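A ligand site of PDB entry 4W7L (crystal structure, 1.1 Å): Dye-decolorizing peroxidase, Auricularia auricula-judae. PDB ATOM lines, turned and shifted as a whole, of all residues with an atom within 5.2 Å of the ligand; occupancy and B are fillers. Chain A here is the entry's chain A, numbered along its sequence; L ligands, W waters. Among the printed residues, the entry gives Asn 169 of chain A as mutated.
NE2 of His 305 binds FE1 of the ligand, at 2.1 Å.
The backbone NH (N) of Gly 170 lies within hydrogen-bond range of an oxygen (O2) of the ligand (2.7 Å).
NH2 of Arg 312 is in salt-bridge range of O3 of the ligand, at 2.8 Å.
The guanidinium group (NH2) of Arg 333 is in salt-bridge range of an oxygen (O2) of the ligand (2.9 Å).
OD1 of Asn 169 sits close to O2 of the ligand (3.0 Å).
The backbone NH (N) of Ala 172 is in hydrogen-bond range of an oxygen (O1) of the ligand, at 3.1 Å.
N of Ile 171 lies within hydrogen-bond range of O2 of the ligand, at 3.3 Å.
The side-chain hydroxyl (OG1) of Thr 309 sits at hydrogen-bond distance from the backbone carbonyl oxygen (O) of His 305 (3.1 Å).
N of His 305 lies within hydrogen-bond range of O of Val 254.
The guanidinium group (NH2) of Arg 312 is in hydrogen-bond range of the side-chain amide oxygen (OD1) of Asn 282 (2.8 Å).
NH1 of Arg 333 lies within hydrogen-bond range of OD1 of Asn 169 (3.1 Å).
NE2 of Gln 173 is in hydrogen-bond range of O of Arg 333 (2.8 Å).
N of Phe 167 lies within hydrogen-bond range of OE1 of Glu 163, at 2.8 Å.
O of Ile 399 lies within hydrogen-bond range of NE2 of Gln 375 (2.9 Å).
The backbone NH (N) of Leu 358 is in hydrogen-bond range of the backbone carbonyl oxygen (O) of Leu 220, 2.8 Å away.
Water W1 lies within hydrogen-bond range of an oxygen (O4) of the ligand (2.8 Å) and the backbone carbonyl oxygen (O) of Ala 172 (3.4 Å).
Water W2 lies within hydrogen-bond range of O of Arg 310, OH of Tyr 286, NE of Arg 312, O3 of the ligand and O of Ile 306.
Water W4 lies within hydrogen-bond range of NH2 of Arg 256 (2.8 Å) and O3 of the ligand (2.9 Å).
Residues that only touch the ligand: Phe 360, Thr 309, Arg 310, Glu 163, Ile 399, Gln 222, Leu 168, Phe 371, Phe 167, Ile 306, Leu 358, Arg 256, Val 254, Val 427, Gln 375, Leu 220, Leu 374, Ile 398, Ile 331 and Phe 165.
Within 4 Å of the ligand: Glu 163, Phe 165, Phe 167, Leu 168, Asn 169, Gly 170, Ile 171, Ala 172, Leu 220, Gln 222, Val 254, Arg 256, His 305, Ile 306, Thr 309, Arg 310, Arg 312, Ile 331, Arg 333, Leu 358, Phe 360, Phe 371, Leu 374, Gln 375, Ile 398, Ile 399 and Val 427.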
ATOM      1  N   GLU A 163     -14.349   6.922 -19.775  1.00  0.00           N
ATOM      2  CA  GLU A 163     -13.268   7.039 -20.734  1.00  0.00           C
ATOM      3  C   GLU A 163     -12.396   5.785 -20.712  1.00  0.00           C
ATOM      4  O   GLU A 163     -12.640   4.871 -19.911  1.00  0.00           O
ATOM      5  CB  GLU A 163     -12.529   8.394 -20.569  1.00  0.00           C
ATOM      6  CG  GLU A 163     -12.020   8.713 -19.192  1.00  0.00           C
ATOM      7  CD  GLU A 163     -10.959   7.738 -18.786  1.00  0.00           C
ATOM      8  OE1 GLU A 163     -11.080   7.096 -17.721  1.00  0.00           O
ATOM      9  OE2 GLU A 163      -9.980   7.608 -19.568  1.00  0.00           O
ATOM     10  N   PHE A 165      -9.448   4.908 -19.588  1.00  0.00           N
ATOM     11  CA  PHE A 165      -8.819   4.452 -18.346  1.00  0.00           C
ATOM     12  C   PHE A 165      -9.838   3.883 -17.369  1.00  0.00           C
ATOM     13  O   PHE A 165      -9.446   3.324 -16.348  1.00  0.00           O
ATOM     14  CB  PHE A 165      -8.072   5.588 -17.624  1.00  0.00           C
ATOM     15  CG  PHE A 165      -6.855   6.124 -18.333  1.00  0.00           C
ATOM     16  CD1 PHE A 165      -5.962   5.316 -18.988  1.00  0.00           C
ATOM     17  CD2 PHE A 165      -6.572   7.487 -18.264  1.00  0.00           C
ATOM     18  CE1 PHE A 165      -4.833   5.848 -19.600  1.00  0.00           C
ATOM     19  CE2 PHE A 165      -5.446   8.035 -18.895  1.00  0.00           C
ATOM     20  CZ  PHE A 165      -4.584   7.203 -19.567  1.00  0.00           C
ATOM     21  N   PHE A 167     -12.708   5.646 -16.012  1.00  0.00           N
ATOM     22  CA  PHE A 167     -13.363   6.603 -15.113  1.00  0.00           C
ATOM     23  C   PHE A 167     -14.595   7.210 -15.775  1.00  0.00           C
ATOM     24  O   PHE A 167     -14.565   7.638 -16.926  1.00  0.00           O
ATOM     25  CB  PHE A 167     -12.412   7.752 -14.748  1.00  0.00           C
ATOM     26  CG  PHE A 167     -11.215   7.312 -13.932  1.00  0.00           C
ATOM     27  CD1 PHE A 167     -10.147   6.662 -14.525  1.00  0.00           C
ATOM     28  CD2 PHE A 167     -11.175   7.529 -12.566  1.00  0.00           C
ATOM     29  CE1 PHE A 167      -9.068   6.209 -13.760  1.00  0.00           C
ATOM     30  CE2 PHE A 167     -10.127   7.074 -11.793  1.00  0.00           C
ATOM     31  CZ  PHE A 167      -9.054   6.415 -12.384  1.00  0.00           C
ATOM     32  N   LEU A 168     -15.675   7.307 -14.992  1.00  0.00           N
ATOM     33  CA  LEU A 168     -16.855   8.007 -15.473  1.00  0.00           C
ATOM     34  C   LEU A 168     -16.465   9.419 -15.849  1.00  0.00           C
ATOM     35  O   LEU A 168     -15.778  10.112 -15.090  1.00  0.00           O
ATOM     36  CB  LEU A 168     -17.907   8.029 -14.371  1.00  0.00           C
ATOM     37  CG  LEU A 168     -19.251   8.635 -14.755  1.00  0.00           C
ATOM     38  CD1 LEU A 168     -19.925   7.904 -15.911  1.00  0.00           C
ATOM     39  CD2 LEU A 168     -20.173   8.677 -13.563  1.00  0.00           C
ATOM     40  N   ASN A 169     -16.910   9.856 -17.027  1.00  0.00           N
ATOM     41  CA  ASN A 169     -16.451  11.112 -17.579  1.00  0.00           C
ATOM     42  C   ASN A 169     -17.691  11.897 -18.031  1.00  0.00           C
ATOM     43  O   ASN A 169     -18.715  11.318 -18.366  1.00  0.00           O
ATOM     44  CB  ASN A 169     -15.510  10.816 -18.735  1.00  0.00           C
ATOM     45  CG  ASN A 169     -14.825  12.031 -19.254  1.00  0.00           C
ATOM     46  OD1 ASN A 169     -14.431  12.919 -18.497  1.00  0.00           O
ATOM     47  ND2 ASN A 169     -14.700  12.094 -20.569  1.00  0.00           N
ATOM     48  N   GLY A 170     -17.583  13.220 -18.068  1.00  0.00           N
ATOM     49  CA  GLY A 170     -18.677  14.094 -18.432  1.00  0.00           C
ATOM     50  C   GLY A 170     -19.555  14.507 -17.252  1.00  0.00           C
ATOM     51  O   GLY A 170     -20.642  15.019 -17.462  1.00  0.00           O
ATOM     52  N   ILE A 171     -19.094  14.286 -16.031  1.00  0.00           N
ATOM     53  CA  ILE A 171     -19.843  14.616 -14.848  1.00  0.00           C
ATOM     54  C   ILE A 171     -19.955  16.126 -14.650  1.00  0.00           C
ATOM     55  O   ILE A 171     -21.032  16.647 -14.375  1.00  0.00           O
ATOM     56  CB  ILE A 171     -19.163  14.004 -13.589  1.00  0.00           C
ATOM     57  CG1 ILE A 171     -19.167  12.471 -13.665  1.00  0.00           C
ATOM     58  CG2 ILE A 171     -19.806  14.503 -12.302  1.00  0.00           C
ATOM     59  CD1 ILE A 171     -18.311  11.781 -12.603  1.00  0.00           C
ATOM     60  N   ALA A 172     -18.820  16.806 -14.751  1.00  0.00           N
ATOM     61  CA  ALA A 172     -18.702  18.176 -14.264  1.00  0.00           C
ATOM     62  C   ALA A 172     -18.597  19.169 -15.399  1.00  0.00           C
ATOM     63  O   ALA A 172     -17.641  19.142 -16.124  1.00  0.00           O
ATOM     64  CB  ALA A 172     -17.493  18.287 -13.369  1.00  0.00           C
ATOM     65  N   GLN A 173     -19.578  20.050 -15.520  1.00  0.00           N
ATOM     66  CA  GLN A 173     -19.604  21.045 -16.575  1.00  0.00           C
ATOM     67  C   GLN A 173     -20.014  22.366 -15.922  1.00  0.00           C
ATOM     68  O   GLN A 173     -20.710  22.365 -14.910  1.00  0.00           O
ATOM     69  CB  GLN A 173     -20.670  20.710 -17.617  1.00  0.00           C
ATOM     70  CG  GLN A 173     -20.525  19.357 -18.273  1.00  0.00           C
ATOM     71  CD  GLN A 173     -19.549  19.313 -19.418  1.00  0.00           C
ATOM     72  OE1 GLN A 173     -18.611  20.098 -19.552  1.00  0.00           O
ATOM     73  NE2 GLN A 173     -19.741  18.323 -20.244  1.00  0.00           N
ATOM     74  N   LEU A 220      -6.273  12.477 -28.306  1.00  0.00           N
ATOM     75  CA  LEU A 220      -5.428  12.160 -27.157  1.00  0.00           C
ATOM     76  C   LEU A 220      -5.399  10.657 -26.963  1.00  0.00           C
ATOM     77  O   LEU A 220      -6.319  10.043 -26.442  1.00  0.00           O
ATOM     78  CB  LEU A 220      -5.939  12.874 -25.916  1.00  0.00           C
ATOM     79  CG  LEU A 220      -5.984  14.411 -26.023  1.00  0.00           C
ATOM     80  CD1 LEU A 220      -6.508  14.995 -24.753  1.00  0.00           C
ATOM     81  CD2 LEU A 220      -4.612  14.969 -26.335  1.00  0.00           C
ATOM     82  N   GLN A 222      -4.470   7.221 -25.245  1.00  0.00           N
ATOM     83  CA  GLN A 222      -4.300   6.768 -23.874  1.00  0.00           C
ATOM     84  C   GLN A 222      -3.637   5.407 -23.853  1.00  0.00           C
ATOM     85  O   GLN A 222      -4.029   4.499 -24.568  1.00  0.00           O
ATOM     86  CB  GLN A 222      -5.638   6.710 -23.184  1.00  0.00           C
ATOM     87  CG  GLN A 222      -6.258   8.095 -23.035  1.00  0.00           C
ATOM     88  CD  GLN A 222      -7.658   8.026 -22.518  1.00  0.00           C
ATOM     89  OE1 GLN A 222      -8.604   8.294 -23.234  1.00  0.00           O
ATOM     90  NE2 GLN A 222      -7.778   7.696 -21.250  1.00  0.00           N
ATOM     91  N   VAL A 254      -6.762  11.271 -10.657  1.00  0.00           N
ATOM     92  CA  VAL A 254      -7.856  11.893 -11.363  1.00  0.00           C
ATOM     93  C   VAL A 254      -8.549  12.936 -10.497  1.00  0.00           C
ATOM     94  O   VAL A 254      -8.965  13.992 -10.994  1.00  0.00           O
ATOM     95  CB  VAL A 254      -8.861  10.817 -11.876  1.00  0.00           C
ATOM     96  CG1 VAL A 254     -10.110  11.454 -12.459  1.00  0.00           C
ATOM     97  CG2 VAL A 254      -8.184   9.936 -12.903  1.00  0.00           C
ATOM     98  N   ARG A 256     -11.236  11.673  -8.810  1.00  0.00           N
ATOM     99  CA  ARG A 256     -12.435  10.886  -8.637  1.00  0.00           C
ATOM    100  C   ARG A 256     -12.071   9.429  -8.750  1.00  0.00           C
ATOM    101  O   ARG A 256     -11.155   9.064  -9.479  1.00  0.00           O
ATOM    102  CB  ARG A 256     -13.475  11.174  -9.724  1.00  0.00           C
ATOM    103  CG  ARG A 256     -13.979  12.586  -9.754  1.00  0.00           C
ATOM    104  CD  ARG A 256     -15.110  12.739 -10.808  1.00  0.00           C
ATOM    105  NE  ARG A 256     -15.588  14.117 -10.838  1.00  0.00           N
ATOM    106  CZ  ARG A 256     -16.536  14.598 -10.033  1.00  0.00           C
ATOM    107  NH1 ARG A 256     -17.208  13.810  -9.210  1.00  0.00           N
ATOM    108  NH2 ARG A 256     -16.802  15.894 -10.054  1.00  0.00           N
ATOM    109  N   ASN A 282     -20.789  16.358  -7.143  1.00  0.00           N
ATOM    110  CA  ASN A 282     -20.016  17.552  -7.457  1.00  0.00           C
ATOM    111  C   ASN A 282     -20.001  18.565  -6.318  1.00  0.00           C
ATOM    112  O   ASN A 282     -19.505  19.676  -6.486  1.00  0.00           O
ATOM    113  CB  ASN A 282     -20.475  18.201  -8.763  1.00  0.00           C
ATOM    114  CG  ASN A 282     -19.313  18.779  -9.537  1.00  0.00           C
ATOM    115  OD1 ASN A 282     -18.167  18.396  -9.330  1.00  0.00           O
ATOM    116  ND2 ASN A 282     -19.612  19.687 -10.468  1.00  0.00           N
ATOM    117  N   TYR A 286     -12.958  21.614  -2.284  1.00  0.00           N
ATOM    118  CA  TYR A 286     -11.595  21.295  -1.801  1.00  0.00           C
ATOM    119  C   TYR A 286     -11.295  21.834  -0.419  1.00  0.00           C
ATOM    120  O   TYR A 286     -10.307  21.432   0.195  1.00  0.00           O
ATOM    121  CB  TYR A 286     -10.467  21.660  -2.782  1.00  0.00           C
ATOM    122  CG  TYR A 286     -10.623  20.949  -4.101  1.00  0.00           C
ATOM    123  CD1 TYR A 286     -10.710  19.567  -4.164  1.00  0.00           C
ATOM    124  CD2 TYR A 286     -10.727  21.664  -5.281  1.00  0.00           C
ATOM    125  CE1 TYR A 286     -10.889  18.907  -5.368  1.00  0.00           C
ATOM    126  CE2 TYR A 286     -10.907  21.024  -6.494  1.00  0.00           C
ATOM    127  CZ  TYR A 286     -11.015  19.643  -6.520  1.00  0.00           C
ATOM    128  OH  TYR A 286     -11.202  18.935  -7.678  1.00  0.00           O
ATOM    129  N   HIS A 305      -6.052  15.702 -11.476  1.00  0.00           N
ATOM    130  CA  HIS A 305      -6.511  16.261 -12.730  1.00  0.00           C
ATOM    131  C   HIS A 305      -7.664  17.245 -12.554  1.00  0.00           C
ATOM    132  O   HIS A 305      -7.619  18.337 -13.075  1.00  0.00           O
ATOM    133  CB  HIS A 305      -6.892  15.121 -13.676  1.00  0.00           C
ATOM    134  CG  HIS A 305      -7.504  15.584 -14.957  1.00  0.00           C
ATOM    135  ND1 HIS A 305      -6.867  16.467 -15.795  1.00  0.00           N
ATOM    136  CD2 HIS A 305      -8.662  15.249 -15.580  1.00  0.00           C
ATOM    137  CE1 HIS A 305      -7.602  16.642 -16.876  1.00  0.00           C
ATOM    138  NE2 HIS A 305      -8.698  15.924 -16.776  1.00  0.00           N
ATOM    139  N   ILE A 306      -8.729  16.867 -11.846  1.00  0.00           N
ATOM    140  CA  ILE A 306      -9.851  17.780 -11.787  1.00  0.00           C
ATOM    141  C   ILE A 306      -9.535  18.998 -10.955  1.00  0.00           C
ATOM    142  O   ILE A 306     -10.142  20.060 -11.162  1.00  0.00           O
ATOM    143  CB  ILE A 306     -11.159  17.086 -11.312  1.00  0.00           C
ATOM    144  CG1 ILE A 306     -11.073  16.558  -9.880  1.00  0.00           C
ATOM    145  CG2 ILE A 306     -11.539  16.019 -12.292  1.00  0.00           C
ATOM    146  CD1 ILE A 306     -12.445  16.304  -9.317  1.00  0.00           C
ATOM    147  N   THR A 309      -7.765  21.393 -13.247  1.00  0.00           N
ATOM    148  CA  THR A 309      -8.553  21.958 -14.330  1.00  0.00           C
ATOM    149  C   THR A 309      -9.767  22.763 -13.882  1.00  0.00           C
ATOM    150  O   THR A 309     -10.243  23.598 -14.634  1.00  0.00           O
ATOM    151  CB  THR A 309      -8.949  20.892 -15.351  1.00  0.00           C
ATOM    152  OG1 THR A 309      -9.722  19.889 -14.701  1.00  0.00           O
ATOM    153  CG2 THR A 309      -7.741  20.288 -16.037  1.00  0.00           C
ATOM    154  N   ARG A 310     -10.273  22.534 -12.665  1.00  0.00           N
ATOM    155  CA  ARG A 310     -11.220  23.446 -12.003  1.00  0.00           C
ATOM    156  C   ARG A 310     -10.775  23.571 -10.559  1.00  0.00           C
ATOM    157  O   ARG A 310     -11.116  22.743  -9.701  1.00  0.00           O
ATOM    158  CB  ARG A 310     -12.668  22.980 -12.087  1.00  0.00           C
ATOM    159  CG  ARG A 310     -13.620  23.986 -11.422  1.00  0.00           C
ATOM    160  CD  ARG A 310     -15.041  23.510 -11.239  1.00  0.00           C
ATOM    161  NE  ARG A 310     -15.760  24.484 -10.425  1.00  0.00           N
ATOM    162  CZ  ARG A 310     -16.836  24.205  -9.693  1.00  0.00           C
ATOM    163  NH1 ARG A 310     -17.428  23.029  -9.756  1.00  0.00           N
ATOM    164  NH2 ARG A 310     -17.333  25.151  -8.907  1.00  0.00           N
ATOM    165  N   ARG A 312     -11.466  25.441  -8.073  1.00  0.00           N
ATOM    166  CA  ARG A 312     -12.426  25.733  -7.001  1.00  0.00           C
ATOM    167  C   ARG A 312     -11.771  26.614  -5.932  1.00  0.00           C
ATOM    168  O   ARG A 312     -11.232  27.670  -6.261  1.00  0.00           O
ATOM    169  CB  ARG A 312     -13.090  24.468  -6.451  1.00  0.00           C
ATOM    170  CG  ARG A 312     -13.702  23.605  -7.536  1.00  0.00           C
ATOM    171  CD  ARG A 312     -14.457  22.405  -7.000  1.00  0.00           C
ATOM    172  NE  ARG A 312     -14.697  21.450  -8.090  1.00  0.00           N
ATOM    173  CZ  ARG A 312     -15.779  20.708  -8.250  1.00  0.00           C
ATOM    174  NH1 ARG A 312     -16.784  20.755  -7.391  1.00  0.00           N
ATOM    175  NH2 ARG A 312     -15.867  19.932  -9.317  1.00  0.00           N
ATOM    176  N   ILE A 331     -14.741  25.415 -19.360  1.00  0.00           N
ATOM    177  CA  ILE A 331     -14.933  24.812 -20.655  1.00  0.00           C
ATOM    178  C   ILE A 331     -16.114  23.851 -20.595  1.00  0.00           C
ATOM    179  O   ILE A 331     -16.365  23.226 -19.579  1.00  0.00           O
ATOM    180  CB  ILE A 331     -13.667  24.081 -21.181  1.00  0.00           C
ATOM    181  CG1 ILE A 331     -13.244  22.923 -20.270  1.00  0.00           C
ATOM    182  CG2 ILE A 331     -12.559  25.080 -21.357  1.00  0.00           C
ATOM    183  CD1 ILE A 331     -12.131  22.079 -20.872  1.00  0.00           C
ATOM    184  N   ARG A 333     -17.181  20.345 -22.099  1.00  0.00           N
ATOM    185  CA  ARG A 333     -16.536  19.204 -22.722  1.00  0.00           C
ATOM    186  C   ARG A 333     -17.540  18.274 -23.369  1.00  0.00           C
ATOM    187  O   ARG A 333     -18.579  17.963 -22.786  1.00  0.00           O
ATOM    188  CB  ARG A 333     -15.771  18.422 -21.669  1.00  0.00           C
ATOM    189  CG  ARG A 333     -14.560  19.180 -21.128  1.00  0.00           C
ATOM    190  CD  ARG A 333     -13.869  18.459 -19.988  1.00  0.00           C
ATOM    191  NE  ARG A 333     -14.782  18.317 -18.859  1.00  0.00           N
ATOM    192  CZ  ARG A 333     -15.082  17.191 -18.229  1.00  0.00           C
ATOM    193  NH1 ARG A 333     -14.502  16.055 -18.563  1.00  0.00           N
ATOM    194  NH2 ARG A 333     -15.992  17.202 -17.282  1.00  0.00           N
ATOM    195  N   LEU A 358      -9.044   9.362 -26.210  1.00  0.00           N
ATOM    196  CA  LEU A 358     -10.145  10.303 -26.068  1.00  0.00           C
ATOM    197  C   LEU A 358     -10.146  11.255 -27.254  1.00  0.00           C
ATOM    198  O   LEU A 358      -9.133  11.917 -27.513  1.00  0.00           O
ATOM    199  CB  LEU A 358     -10.022  11.097 -24.770  1.00  0.00           C
ATOM    200  CG  LEU A 358     -11.194  12.034 -24.457  1.00  0.00           C
ATOM    201  CD1 LEU A 358     -12.513  11.268 -24.271  1.00  0.00           C
ATOM    202  CD2 LEU A 358     -10.882  12.861 -23.232  1.00  0.00           C
ATOM    203  N   PHE A 360     -11.107  14.399 -27.704  1.00  0.00           N
ATOM    204  CA  PHE A 360     -11.380  15.465 -26.770  1.00  0.00           C
ATOM    205  C   PHE A 360     -11.958  16.655 -27.510  1.00  0.00           C
ATOM    206  O   PHE A 360     -11.418  17.078 -28.542  1.00  0.00           O
ATOM    207  CB  PHE A 360     -10.074  15.829 -26.031  1.00  0.00           C
ATOM    208  CG  PHE A 360     -10.188  17.035 -25.158  1.00  0.00           C
ATOM    209  CD1 PHE A 360      -9.941  18.303 -25.676  1.00  0.00           C
ATOM    210  CD2 PHE A 360     -10.479  16.921 -23.823  1.00  0.00           C
ATOM    211  CE1 PHE A 360     -10.027  19.422 -24.890  1.00  0.00           C
ATOM    212  CE2 PHE A 360     -10.551  18.039 -23.028  1.00  0.00           C
ATOM    213  CZ  PHE A 360     -10.314  19.299 -23.552  1.00  0.00           C
ATOM    214  N   PHE A 371      -9.470  25.962 -22.966  1.00  0.00           N
ATOM    215  CA  PHE A 371      -8.587  24.825 -23.144  1.00  0.00           C
ATOM    216  C   PHE A 371      -7.097  25.216 -23.067  1.00  0.00           C
ATOM    217  O   PHE A 371      -6.305  24.564 -22.369  1.00  0.00           O
ATOM    218  CB  PHE A 371      -8.869  24.118 -24.486  1.00  0.00           C
ATOM    219  CG  PHE A 371      -7.728  23.275 -24.926  1.00  0.00           C
ATOM    220  CD1 PHE A 371      -7.406  22.105 -24.259  1.00  0.00           C
ATOM    221  CD2 PHE A 371      -6.903  23.695 -25.943  1.00  0.00           C
ATOM    222  CE1 PHE A 371      -6.294  21.366 -24.629  1.00  0.00           C
ATOM    223  CE2 PHE A 371      -5.808  22.973 -26.307  1.00  0.00           C
ATOM    224  CZ  PHE A 371      -5.491  21.812 -25.643  1.00  0.00           C
ATOM    225  N   LEU A 374      -6.063  26.102 -19.392  1.00  0.00           N
ATOM    226  CA  LEU A 374      -6.051  24.951 -18.519  1.00  0.00           C
ATOM    227  C   LEU A 374      -4.831  24.082 -18.783  1.00  0.00           C
ATOM    228  O   LEU A 374      -4.203  23.607 -17.834  1.00  0.00           O
ATOM    229  CB  LEU A 374      -7.336  24.143 -18.711  1.00  0.00           C
ATOM    230  CG  LEU A 374      -8.506  24.559 -17.834  1.00  0.00           C
ATOM    231  CD1 LEU A 374      -8.815  26.037 -17.853  1.00  0.00           C
ATOM    232  CD2 LEU A 374      -9.756  23.759 -18.226  1.00  0.00           C
ATOM    233  N   GLN A 375      -4.505  23.856 -20.047  1.00  0.00           N
ATOM    234  CA  GLN A 375      -3.400  23.007 -20.377  1.00  0.00           C
ATOM    235  C   GLN A 375      -2.059  23.676 -19.987  1.00  0.00           C
ATOM    236  O   GLN A 375      -1.230  23.069 -19.293  1.00  0.00           O
ATOM    237  CB  GLN A 375      -3.408  22.677 -21.876  1.00  0.00           C
ATOM    238  CG  GLN A 375      -2.294  21.708 -22.287  1.00  0.00           C
ATOM    239  CD  GLN A 375      -2.565  20.289 -21.818  1.00  0.00           C
ATOM    240  OE1 GLN A 375      -3.586  19.694 -22.135  1.00  0.00           O
ATOM    241  NE2 GLN A 375      -1.618  19.735 -21.060  1.00  0.00           N
ATOM    242  N   ILE A 398      -2.568  13.186 -15.438  1.00  0.00           N
ATOM    243  CA  ILE A 398      -3.313  12.703 -16.594  1.00  0.00           C
ATOM    244  C   ILE A 398      -2.879  13.425 -17.867  1.00  0.00           C
ATOM    245  O   ILE A 398      -2.574  12.766 -18.861  1.00  0.00           O
ATOM    246  CB  ILE A 398      -4.828  12.823 -16.344  1.00  0.00           C
ATOM    247  CG1 ILE A 398      -5.236  12.088 -15.047  1.00  0.00           C
ATOM    248  CG2 ILE A 398      -5.627  12.297 -17.537  1.00  0.00           C
ATOM    249  CD1 ILE A 398      -4.846  10.599 -14.950  1.00  0.00           C
ATOM    250  N   ILE A 399      -2.878  14.757 -17.844  1.00  0.00           N
ATOM    251  CA  ILE A 399      -2.638  15.520 -19.065  1.00  0.00           C
ATOM    252  C   ILE A 399      -1.396  16.393 -19.063  1.00  0.00           C
ATOM    253  O   ILE A 399      -1.092  17.017 -20.065  1.00  0.00           O
ATOM    254  CB  ILE A 399      -3.857  16.403 -19.444  1.00  0.00           C
ATOM    255  CG1 ILE A 399      -4.140  17.470 -18.385  1.00  0.00           C
ATOM    256  CG2 ILE A 399      -5.083  15.530 -19.706  1.00  0.00           C
ATOM    257  CD1 ILE A 399      -5.024  18.597 -18.850  1.00  0.00           C
ATOM    258  N   VAL A 427      -1.001   9.796 -21.518  1.00  0.00           N
ATOM    259  CA  VAL A 427      -1.808  10.411 -22.566  1.00  0.00           C
ATOM    260  C   VAL A 427      -0.819  11.026 -23.536  1.00  0.00           C
ATOM    261  O   VAL A 427       0.093  11.752 -23.114  1.00  0.00           O
ATOM    262  CB  VAL A 427      -2.745  11.489 -21.993  1.00  0.00           C
ATOM    263  CG1 VAL A 427      -3.466  12.211 -23.116  1.00  0.00           C
ATOM    264  CG2 VAL A 427      -3.746  10.866 -21.061  1.00  0.00           C
HETATM  265  C1  LIG L   1     -12.664  16.110 -15.740  1.00  0.00           C
HETATM  266  C2  LIG L   1     -10.399  12.409 -17.868  1.00  0.00           C
HETATM  267  C3  LIG L   1      -8.258  15.492 -20.914  1.00  0.00           C
HETATM  268  C4  LIG L   1     -10.301  19.212 -18.580  1.00  0.00           C
HETATM  269  C5  LIG L   1     -12.251  14.833 -16.034  1.00  0.00           C
HETATM  270  C6  LIG L   1     -12.633  13.617 -15.359  1.00  0.00           C
HETATM  271  C7  LIG L   1     -12.020  12.599 -15.955  1.00  0.00           C
HETATM  272  C8  LIG L   1     -11.217  13.134 -17.021  1.00  0.00           C
HETATM  273  C9  LIG L   1     -12.131  11.115 -15.654  1.00  0.00           C
HETATM  274  C10 LIG L   1     -13.574  13.558 -14.151  1.00  0.00           C
HETATM  275  C11 LIG L   1     -15.070  13.431 -14.460  1.00  0.00           C
HETATM  276  C12 LIG L   1     -15.660  14.605 -15.157  1.00  0.00           C
HETATM  277  O1  LIG L   1     -15.952  15.644 -14.542  1.00  0.00           O
HETATM  278  O2  LIG L   1     -15.866  14.461 -16.392  1.00  0.00           O
HETATM  279  C13 LIG L   1      -9.600  12.928 -18.870  1.00  0.00           C
HETATM  280  C14 LIG L   1      -8.783  12.161 -19.765  1.00  0.00           C
HETATM  281  C15 LIG L   1      -8.205  13.005 -20.618  1.00  0.00           C
HETATM  282  C16 LIG L   1      -8.673  14.338 -20.283  1.00  0.00           C
HETATM  283  C17 LIG L   1      -8.573  10.647 -19.655  1.00  0.00           C
HETATM  284  C18 LIG L   1      -7.228  12.724 -21.755  1.00  0.00           C
HETATM  285  C19 LIG L   1      -7.227  11.565 -22.450  1.00  0.00           C
HETATM  286  C20 LIG L   1      -8.563  16.795 -20.518  1.00  0.00           C
HETATM  287  C21 LIG L   1      -8.022  18.003 -21.063  1.00  0.00           C
HETATM  288  C22 LIG L   1      -8.549  19.026 -20.385  1.00  0.00           C
HETATM  289  C23 LIG L   1      -9.474  18.490 -19.430  1.00  0.00           C
HETATM  290  C24 LIG L   1      -7.022  18.031 -22.212  1.00  0.00           C
HETATM  291  C25 LIG L   1      -8.298  20.511 -20.534  1.00  0.00           C
HETATM  292  C26 LIG L   1      -7.144  21.015 -20.960  1.00  0.00           C
HETATM  293  C27 LIG L   1     -11.173  18.682 -17.659  1.00  0.00           C
HETATM  294  C28 LIG L   1     -12.075  19.475 -16.895  1.00  0.00           C
HETATM  295  C29 LIG L   1     -12.788  18.567 -16.042  1.00  0.00           C
HETATM  296  C30 LIG L   1     -12.261  17.274 -16.361  1.00  0.00           C
HETATM  297  C31 LIG L   1     -12.308  20.983 -16.952  1.00  0.00           C
HETATM  298  C32 LIG L   1     -13.835  18.935 -15.022  1.00  0.00           C
HETATM  299  C33 LIG L   1     -13.225  19.583 -13.793  1.00  0.00           C
HETATM  300  C34 LIG L   1     -14.277  20.008 -12.809  1.00  0.00           C
HETATM  301  O3  LIG L   1     -14.223  19.582 -11.618  1.00  0.00           O
HETATM  302  O4  LIG L   1     -15.178  20.794 -13.191  1.00  0.00           O
HETATM  303  N1  LIG L   1     -11.359  14.512 -17.047  1.00  0.00           N
HETATM  304  N2  LIG L   1      -9.540  14.246 -19.219  1.00  0.00           N
HETATM  305  N3  LIG L   1      -9.439  17.116 -19.496  1.00  0.00           N
HETATM  306  N4  LIG L   1     -11.310  17.363 -17.362  1.00  0.00           N
HETATM  307 FE1  LIG L   1     -10.283  15.825 -18.154  1.00  0.00          FE
HETATM  308  O   HOH W   1     -15.879  22.029 -15.548  1.00  0.00           O
HETATM  309  O   HOH W   2     -12.518  20.427  -9.546  1.00  0.00           O
HETATM  310  O   HOH W   3     -17.491  21.216 -11.858  1.00  0.00           O
HETATM  311  O   HOH W   4     -14.887  16.800 -11.924  1.00  0.00           O
